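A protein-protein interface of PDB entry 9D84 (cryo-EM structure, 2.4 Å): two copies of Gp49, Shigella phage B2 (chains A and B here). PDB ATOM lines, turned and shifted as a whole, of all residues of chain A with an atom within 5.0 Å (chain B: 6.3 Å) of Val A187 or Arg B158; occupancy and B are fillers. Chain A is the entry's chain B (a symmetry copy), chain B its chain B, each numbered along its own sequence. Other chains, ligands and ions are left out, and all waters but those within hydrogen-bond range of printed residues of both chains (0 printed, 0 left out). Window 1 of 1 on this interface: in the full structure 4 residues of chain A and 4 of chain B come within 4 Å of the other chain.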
ATOM      1  N   PRO A 125       3.678   8.059 -29.434  1.00  0.00           N
ATOM      2  CA  PRO A 125       2.297   8.451 -29.747  1.00  0.00           C
ATOM      3  C   PRO A 125       1.743   7.615 -30.890  1.00  0.00           C
ATOM      4  O   PRO A 125       2.348   7.520 -31.961  1.00  0.00           O
ATOM      5  CB  PRO A 125       2.415   9.930 -30.135  1.00  0.00           C
ATOM      6  CG  PRO A 125       3.852  10.158 -30.454  1.00  0.00           C
ATOM      7  CD  PRO A 125       4.675   9.009 -29.957  1.00  0.00           C
ATOM      8  N   PHE A 126       0.583   7.006 -30.655  1.00  0.00           N
ATOM      9  CA  PHE A 126      -0.107   6.204 -31.656  1.00  0.00           C
ATOM     10  C   PHE A 126      -1.427   6.883 -31.985  1.00  0.00           C
ATOM     11  O   PHE A 126      -2.239   7.135 -31.090  1.00  0.00           O
ATOM     12  CB  PHE A 126      -0.339   4.777 -31.154  1.00  0.00           C
ATOM     13  CG  PHE A 126      -1.078   3.905 -32.126  1.00  0.00           C
ATOM     14  CD1 PHE A 126      -0.454   3.434 -33.268  1.00  0.00           C
ATOM     15  CD2 PHE A 126      -2.396   3.548 -31.895  1.00  0.00           C
ATOM     16  CE1 PHE A 126      -1.131   2.628 -34.163  1.00  0.00           C
ATOM     17  CE2 PHE A 126      -3.077   2.743 -32.786  1.00  0.00           C
ATOM     18  CZ  PHE A 126      -2.445   2.283 -33.920  1.00  0.00           C
ATOM     19  N   VAL A 127      -1.640   7.175 -33.264  1.00  0.00           N
ATOM     20  CA  VAL A 127      -2.836   7.865 -33.729  1.00  0.00           C
ATOM     21  C   VAL A 127      -3.801   6.832 -34.288  1.00  0.00           C
ATOM     22  O   VAL A 127      -3.453   6.074 -35.200  1.00  0.00           O
ATOM     23  CB  VAL A 127      -2.488   8.927 -34.786  1.00  0.00           C
ATOM     24  CG1 VAL A 127      -3.733   9.687 -35.197  1.00  0.00           C
ATOM     25  CG2 VAL A 127      -1.427   9.876 -34.254  1.00  0.00           C
ATOM     26  N   GLU A 151      -1.620   6.999 -21.266  1.00  0.00           N
ATOM     27  CA  GLU A 151      -2.443   8.157 -21.584  1.00  0.00           C
ATOM     28  C   GLU A 151      -3.189   7.949 -22.893  1.00  0.00           C
ATOM     29  O   GLU A 151      -2.695   7.280 -23.804  1.00  0.00           O
ATOM     30  CB  GLU A 151      -1.591   9.428 -21.687  1.00  0.00           C
ATOM     31  CG  GLU A 151      -0.874   9.803 -20.405  1.00  0.00           C
ATOM     32  CD  GLU A 151      -0.001  11.029 -20.568  1.00  0.00           C
ATOM     33  OE1 GLU A 151       0.168  11.491 -21.715  1.00  0.00           O
ATOM     34  OE2 GLU A 151       0.517  11.533 -19.548  1.00  0.00           O
ATOM     35  N   ILE A 152      -4.382   8.534 -22.971  1.00  0.00           N
ATOM     36  CA  ILE A 152      -5.174   8.599 -24.193  1.00  0.00           C
ATOM     37  C   ILE A 152      -5.593  10.044 -24.392  1.00  0.00           C
ATOM     38  O   ILE A 152      -6.072  10.691 -23.451  1.00  0.00           O
ATOM     39  CB  ILE A 152      -6.406   7.677 -24.134  1.00  0.00           C
ATOM     40  CG1 ILE A 152      -5.977   6.213 -24.095  1.00  0.00           C
ATOM     41  CG2 ILE A 152      -7.315   7.919 -25.322  1.00  0.00           C
ATOM     42  CD1 ILE A 152      -5.170   5.794 -25.277  1.00  0.00           C
ATOM     43  N   TYR A 153      -5.405  10.559 -25.602  1.00  0.00           N
ATOM     44  CA  TYR A 153      -5.768  11.932 -25.933  1.00  0.00           C
ATOM     45  C   TYR A 153      -6.909  11.910 -26.943  1.00  0.00           C
ATOM     46  O   TYR A 153      -6.677  11.781 -28.149  1.00  0.00           O
ATOM     47  CB  TYR A 153      -4.564  12.695 -26.475  1.00  0.00           C
ATOM     48  CG  TYR A 153      -3.552  13.054 -25.413  1.00  0.00           C
ATOM     49  CD1 TYR A 153      -3.697  14.204 -24.649  1.00  0.00           C
ATOM     50  CD2 TYR A 153      -2.452  12.241 -25.171  1.00  0.00           C
ATOM     51  CE1 TYR A 153      -2.773  14.537 -23.682  1.00  0.00           C
ATOM     52  CE2 TYR A 153      -1.526  12.567 -24.202  1.00  0.00           C
ATOM     53  CZ  TYR A 153      -1.692  13.715 -23.460  1.00  0.00           C
ATOM     54  OH  TYR A 153      -0.772  14.045 -22.492  1.00  0.00           O
ATOM     55  N   VAL A 154      -8.135  12.040 -26.450  1.00  0.00           N
ATOM     56  CA  VAL A 154      -9.325  12.098 -27.289  1.00  0.00           C
ATOM     57  C   VAL A 154      -9.651  13.562 -27.534  1.00  0.00           C
ATOM     58  O   VAL A 154     -10.103  14.264 -26.621  1.00  0.00           O
ATOM     59  CB  VAL A 154     -10.511  11.373 -26.636  1.00  0.00           C
ATOM     60  CG1 VAL A 154     -11.757  11.518 -27.496  1.00  0.00           C
ATOM     61  CG2 VAL A 154     -10.181   9.910 -26.413  1.00  0.00           C
ATOM     62  N   GLY A 156      -7.672  16.079 -27.913  1.00  0.00           N
ATOM     63  CA  GLY A 156      -6.861  16.919 -27.057  1.00  0.00           C
ATOM     64  C   GLY A 156      -7.109  16.757 -25.576  1.00  0.00           C
ATOM     65  O   GLY A 156      -6.520  17.499 -24.783  1.00  0.00           O
ATOM     66  N   GLU A 185     -10.434  12.279 -33.071  1.00  0.00           N
ATOM     67  CA  GLU A 185      -8.982  12.165 -33.039  1.00  0.00           C
ATOM     68  C   GLU A 185      -8.551  11.597 -31.695  1.00  0.00           C
ATOM     69  O   GLU A 185      -8.705  12.252 -30.660  1.00  0.00           O
ATOM     70  CB  GLU A 185      -8.331  13.525 -33.280  1.00  0.00           C
ATOM     71  CG  GLU A 185      -6.817  13.507 -33.169  1.00  0.00           C
ATOM     72  CD  GLU A 185      -6.276  14.698 -32.404  1.00  0.00           C
ATOM     73  OE1 GLU A 185      -6.345  14.684 -31.156  1.00  0.00           O
ATOM     74  OE2 GLU A 185      -5.780  15.646 -33.047  1.00  0.00           O
ATOM     75  N   VAL A 186      -8.013  10.382 -31.710  1.00  0.00           N
ATOM     76  CA  VAL A 186      -7.539   9.715 -30.505  1.00  0.00           C
ATOM     77  C   VAL A 186      -6.056   9.432 -30.681  1.00  0.00           C
ATOM     78  O   VAL A 186      -5.664   8.682 -31.583  1.00  0.00           O
ATOM     79  CB  VAL A 186      -8.314   8.421 -30.224  1.00  0.00           C
ATOM     80  CG1 VAL A 186      -7.697   7.679 -29.051  1.00  0.00           C
ATOM     81  CG2 VAL A 186      -9.772   8.734 -29.953  1.00  0.00           C
ATOM     82  N   VAL A 187      -5.237  10.030 -29.825  1.00  0.00           N
ATOM     83  CA  VAL A 187      -3.796   9.812 -29.827  1.00  0.00           C
ATOM     84  C   VAL A 187      -3.471   8.925 -28.635  1.00  0.00           C
ATOM     85  O   VAL A 187      -3.641   9.330 -27.481  1.00  0.00           O
ATOM     86  CB  VAL A 187      -3.019  11.132 -29.773  1.00  0.00           C
ATOM     87  CG1 VAL A 187      -1.526  10.858 -29.705  1.00  0.00           C
ATOM     88  CG2 VAL A 187      -3.354  11.991 -30.982  1.00  0.00           C
ATOM     89  N   LEU A 188      -3.004   7.713 -28.913  1.00  0.00           N
ATOM     90  CA  LEU A 188      -2.697   6.746 -27.872  1.00  0.00           C
ATOM     91  C   LEU A 188      -1.212   6.803 -27.536  1.00  0.00           C
ATOM     92  O   LEU A 188      -0.364   6.670 -28.421  1.00  0.00           O
ATOM     93  CB  LEU A 188      -3.082   5.334 -28.312  1.00  0.00           C
ATOM     94  CG  LEU A 188      -4.551   5.066 -28.654  1.00  0.00           C
ATOM     95  CD1 LEU A 188      -4.855   5.350 -30.115  1.00  0.00           C
ATOM     96  CD2 LEU A 188      -4.920   3.639 -28.286  1.00  0.00           C
ATOM     97  N   MET A 189      -0.907   7.004 -26.259  1.00  0.00           N
ATOM     98  CA  MET A 189       0.468   6.970 -25.779  1.00  0.00           C
ATOM     99  C   MET A 189       0.830   5.536 -25.419  1.00  0.00           C
ATOM    100  O   MET A 189       0.194   4.929 -24.554  1.00  0.00           O
ATOM    101  CB  MET A 189       0.649   7.889 -24.576  1.00  0.00           C
ATOM    102  CG  MET A 189       0.422   9.348 -24.891  1.00  0.00           C
ATOM    103  SD  MET A 189       1.449   9.854 -26.278  1.00  0.00           S
ATOM    104  CE  MET A 189       2.146  11.360 -25.625  1.00  0.00           C
ATOM    105  N   PRO B 150       7.344  17.930 -31.558  1.00  0.00           N
ATOM    106  CA  PRO B 150       6.370  16.847 -31.631  1.00  0.00           C
ATOM    107  C   PRO B 150       4.962  17.230 -31.235  1.00  0.00           C
ATOM    108  O   PRO B 150       4.008  16.594 -31.716  1.00  0.00           O
ATOM    109  CB  PRO B 150       6.987  15.870 -30.622  1.00  0.00           C
ATOM    110  CG  PRO B 150       7.642  16.759 -29.597  1.00  0.00           C
ATOM    111  CD  PRO B 150       8.294  17.811 -30.464  1.00  0.00           C
ATOM    112  N   GLU B 151       4.823  18.253 -30.394  1.00  0.00           N
ATOM    113  CA  GLU B 151       3.523  18.628 -29.857  1.00  0.00           C
ATOM    114  C   GLU B 151       3.390  20.140 -29.770  1.00  0.00           C
ATOM    115  O   GLU B 151       4.373  20.850 -29.546  1.00  0.00           O
ATOM    116  CB  GLU B 151       3.304  18.021 -28.467  1.00  0.00           C
ATOM    117  CG  GLU B 151       3.310  16.506 -28.440  1.00  0.00           C
ATOM    118  CD  GLU B 151       3.148  15.951 -27.040  1.00  0.00           C
ATOM    119  OE1 GLU B 151       3.190  16.745 -26.078  1.00  0.00           O
ATOM    120  OE2 GLU B 151       2.979  14.721 -26.902  1.00  0.00           O
ATOM    121  N   ILE B 152       2.160  20.618 -29.946  1.00  0.00           N
ATOM    122  CA  ILE B 152       1.794  22.012 -29.731  1.00  0.00           C
ATOM    123  C   ILE B 152       0.566  22.031 -28.837  1.00  0.00           C
ATOM    124  O   ILE B 152      -0.396  21.294 -29.083  1.00  0.00           O
ATOM    125  CB  ILE B 152       1.516  22.748 -31.054  1.00  0.00           C
ATOM    126  CG1 ILE B 152       2.794  22.865 -31.879  1.00  0.00           C
ATOM    127  CG2 ILE B 152       0.940  24.126 -30.793  1.00  0.00           C
ATOM    128  CD1 ILE B 152       3.889  23.604 -31.186  1.00  0.00           C
ATOM    129  N   TYR B 153       0.599  22.857 -27.797  1.00  0.00           N
ATOM    130  CA  TYR B 153      -0.513  22.981 -26.862  1.00  0.00           C
ATOM    131  C   TYR B 153      -1.113  24.376 -26.993  1.00  0.00           C
ATOM    132  O   TYR B 153      -0.620  25.330 -26.385  1.00  0.00           O
ATOM    133  CB  TYR B 153      -0.054  22.707 -25.434  1.00  0.00           C
ATOM    134  CG  TYR B 153       0.220  21.249 -25.158  1.00  0.00           C
ATOM    135  CD1 TYR B 153      -0.806  20.389 -24.790  1.00  0.00           C
ATOM    136  CD2 TYR B 153       1.502  20.728 -25.270  1.00  0.00           C
ATOM    137  CE1 TYR B 153      -0.561  19.056 -24.534  1.00  0.00           C
ATOM    138  CE2 TYR B 153       1.754  19.395 -25.018  1.00  0.00           C
ATOM    139  CZ  TYR B 153       0.719  18.564 -24.652  1.00  0.00           C
ATOM    140  OH  TYR B 153       0.964  17.234 -24.400  1.00  0.00           O
ATOM    141  N   VAL B 154      -2.177  24.487 -27.781  1.00  0.00           N
ATOM    142  CA  VAL B 154      -2.901  25.739 -27.962  1.00  0.00           C
ATOM    143  C   VAL B 154      -4.064  25.751 -26.984  1.00  0.00           C
ATOM    144  O   VAL B 154      -5.040  25.011 -27.163  1.00  0.00           O
ATOM    145  CB  VAL B 154      -3.396  25.900 -29.406  1.00  0.00           C
ATOM    146  CG1 VAL B 154      -4.213  27.174 -29.546  1.00  0.00           C
ATOM    147  CG2 VAL B 154      -2.225  25.906 -30.371  1.00  0.00           C
ATOM    148  N   GLY B 156      -4.255  24.565 -23.993  1.00  0.00           N
ATOM    149  CA  GLY B 156      -4.406  23.260 -23.384  1.00  0.00           C
ATOM    150  C   GLY B 156      -4.772  22.147 -24.338  1.00  0.00           C
ATOM    151  O   GLY B 156      -5.005  21.021 -23.885  1.00  0.00           O
ATOM    152  N   PHE B 157      -4.827  22.422 -25.636  1.00  0.00           N
ATOM    153  CA  PHE B 157      -5.174  21.433 -26.645  1.00  0.00           C
ATOM    154  C   PHE B 157      -3.912  20.922 -27.322  1.00  0.00           C
ATOM    155  O   PHE B 157      -3.202  21.682 -27.986  1.00  0.00           O
ATOM    156  CB  PHE B 157      -6.104  22.034 -27.701  1.00  0.00           C
ATOM    157  CG  PHE B 157      -7.502  22.251 -27.221  1.00  0.00           C
ATOM    158  CD1 PHE B 157      -8.156  21.280 -26.492  1.00  0.00           C
ATOM    159  CD2 PHE B 157      -8.163  23.434 -27.496  1.00  0.00           C
ATOM    160  CE1 PHE B 157      -9.443  21.481 -26.054  1.00  0.00           C
ATOM    161  CE2 PHE B 157      -9.449  23.640 -27.056  1.00  0.00           C
ATOM    162  CZ  PHE B 157     -10.089  22.663 -26.331  1.00  0.00           C
ATOM    163  N   ARG B 158      -3.641  19.630 -27.165  1.00  0.00           N
ATOM    164  CA  ARG B 158      -2.488  19.023 -27.815  1.00  0.00           C
ATOM    165  C   ARG B 158      -2.749  18.923 -29.311  1.00  0.00           C
ATOM    166  O   ARG B 158      -3.818  18.471 -29.733  1.00  0.00           O
ATOM    167  CB  ARG B 158      -2.196  17.644 -27.233  1.00  0.00           C
ATOM    168  CG  ARG B 158      -0.886  17.059 -27.726  1.00  0.00           C
ATOM    169  CD  ARG B 158      -0.962  15.555 -27.866  1.00  0.00           C
ATOM    170  NE  ARG B 158       0.284  14.991 -28.367  1.00  0.00           N
ATOM    171  CZ  ARG B 158       0.461  14.558 -29.606  1.00  0.00           C
ATOM    172  NH1 ARG B 158      -0.509  14.616 -30.503  1.00  0.00           N
ATOM    173  NH2 ARG B 158       1.641  14.055 -29.955  1.00  0.00           N
ATOM    174  N   GLN B 159      -1.775  19.342 -30.111  1.00  0.00           N
ATOM    175  CA  GLN B 159      -1.850  19.249 -31.562  1.00  0.00           C
ATOM    176  C   GLN B 159      -0.803  18.261 -32.049  1.00  0.00           C
ATOM    177  O   GLN B 159       0.300  18.194 -31.496  1.00  0.00           O
ATOM    178  CB  GLN B 159      -1.647  20.617 -32.214  1.00  0.00           C
ATOM    179  CG  GLN B 159      -2.386  21.742 -31.517  1.00  0.00           C
ATOM    180  CD  GLN B 159      -3.887  21.634 -31.676  1.00  0.00           C
ATOM    181  OE1 GLN B 159      -4.382  21.170 -32.701  1.00  0.00           O
ATOM    182  NE2 GLN B 159      -4.621  22.065 -30.659  1.00  0.00           N
ATOM    183  N   GLN B 160      -1.156  17.487 -33.069  1.00  0.00           N
ATOM    184  CA  GLN B 160      -0.251  16.494 -33.622  1.00  0.00           C
ATOM    185  C   GLN B 160       0.444  17.039 -34.864  1.00  0.00           C
ATOM    186  O   GLN B 160      -0.116  17.847 -35.611  1.00  0.00           O
ATOM    187  CB  GLN B 160      -1.014  15.210 -33.953  1.00  0.00           C
ATOM    188  CG  GLN B 160      -0.184  14.130 -34.628  1.00  0.00           C
ATOM    189  CD  GLN B 160       0.727  13.405 -33.661  1.00  0.00           C
ATOM    190  OE1 GLN B 160       0.583  13.529 -32.446  1.00  0.00           O
ATOM    191  NE2 GLN B 160       1.675  12.647 -34.196  1.00  0.00           N
ATOM    192  N   VAL B 161       1.687  16.598 -35.070  1.00  0.00           N
ATOM    193  CA  VAL B 161       2.444  16.991 -36.252  1.00  0.00           C
ATOM    194  C   VAL B 161       1.693  16.575 -37.514  1.00  0.00           C
ATOM    195  O   VAL B 161       1.267  15.429 -37.674  1.00  0.00           O
ATOM    196  CB  VAL B 161       3.860  16.389 -36.227  1.00  0.00           C
ATOM    197  CG1 VAL B 161       4.779  17.232 -35.373  1.00  0.00           C
ATOM    198  CG2 VAL B 161       3.818  14.959 -35.710  1.00  0.00           C
ATOM    199  N   ARG B 163      -1.206  17.507 -38.440  1.00  0.00           N
ATOM    200  CA  ARG B 163      -2.632  17.751 -38.265  1.00  0.00           C
ATOM    201  C   ARG B 163      -2.934  19.168 -37.797  1.00  0.00           C
ATOM    202  O   ARG B 163      -3.655  19.904 -38.476  1.00  0.00           O
ATOM    203  CB  ARG B 163      -3.220  16.741 -37.273  1.00  0.00           C
ATOM    204  CG  ARG B 163      -2.655  15.339 -37.400  1.00  0.00           C
ATOM    205  CD  ARG B 163      -3.566  14.319 -36.731  1.00  0.00           C
ATOM    206  NE  ARG B 163      -4.981  14.618 -36.930  1.00  0.00           N
ATOM    207  CZ  ARG B 163      -5.622  14.519 -38.088  1.00  0.00           C
ATOM    208  NH1 ARG B 163      -5.010  14.104 -39.185  1.00  0.00           N
ATOM    209  NH2 ARG B 163      -6.912  14.838 -38.144  1.00  0.00           N
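Gly B156 touches its own counterpart, Gly A156.
Positions printed for both chains: 151, 152, 153, 154 and 156.
Of the 3 pairs that touch across the chains among the printed residues, 1 has its exchanged pair printed and touching as well.
Among the printed residues, merely in contact across the chains: Gly A156 with Gly B156, Val A187 with Arg B158 and Met A189 with Glu B151.
Pro A125 touches none of the printed residues of chain B.
Of chain B, only Arg B158 comes within 4 Å of Val A187.
Of the printed residues of chain B, Met A189 touches Glu B151.
Of the printed residues of chain A, Glu B151 touches Met A189 (3.7 Å).
Of chain A, only Val A187 (3.9 Å) comes within 4 Å of Arg B158.
Printed residues of chain B that touch a printed residue of chain A: Glu B151, Gly B156 and Arg B158.
Of the 13 printed residues of chain A, 3 touch a printed residue of chain B.
Hydrophobic or aromatic side chains of chain A within 4 Å of the printed part of chain B: Val A187 and Met A189.
Among the printed residues, no Asp or Glu carboxylate lies within 4 Å of a Lys or Arg side-chain nitrogen of the other chain.
OE2 of Glu B151 is in salt-bridge range of NE of Arg B158, at 3.1 Å.
OE1 of Glu B151 is in hydrogen-bond range of OH of Tyr B153 (2.8 Å).
O of Tyr A153 lies within hydrogen-bond range of N of Val A187, 2.8 Å away.
The backbone carbonyl oxygen (O) of Glu A151 lies within hydrogen-bond range of the backbone NH (N) of Met A189 (3.0 Å).
The guanidinium group (NH1) of Arg B158 lies within hydrogen-bond range of the side-chain amide oxygen (OE1) of Gln B160.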
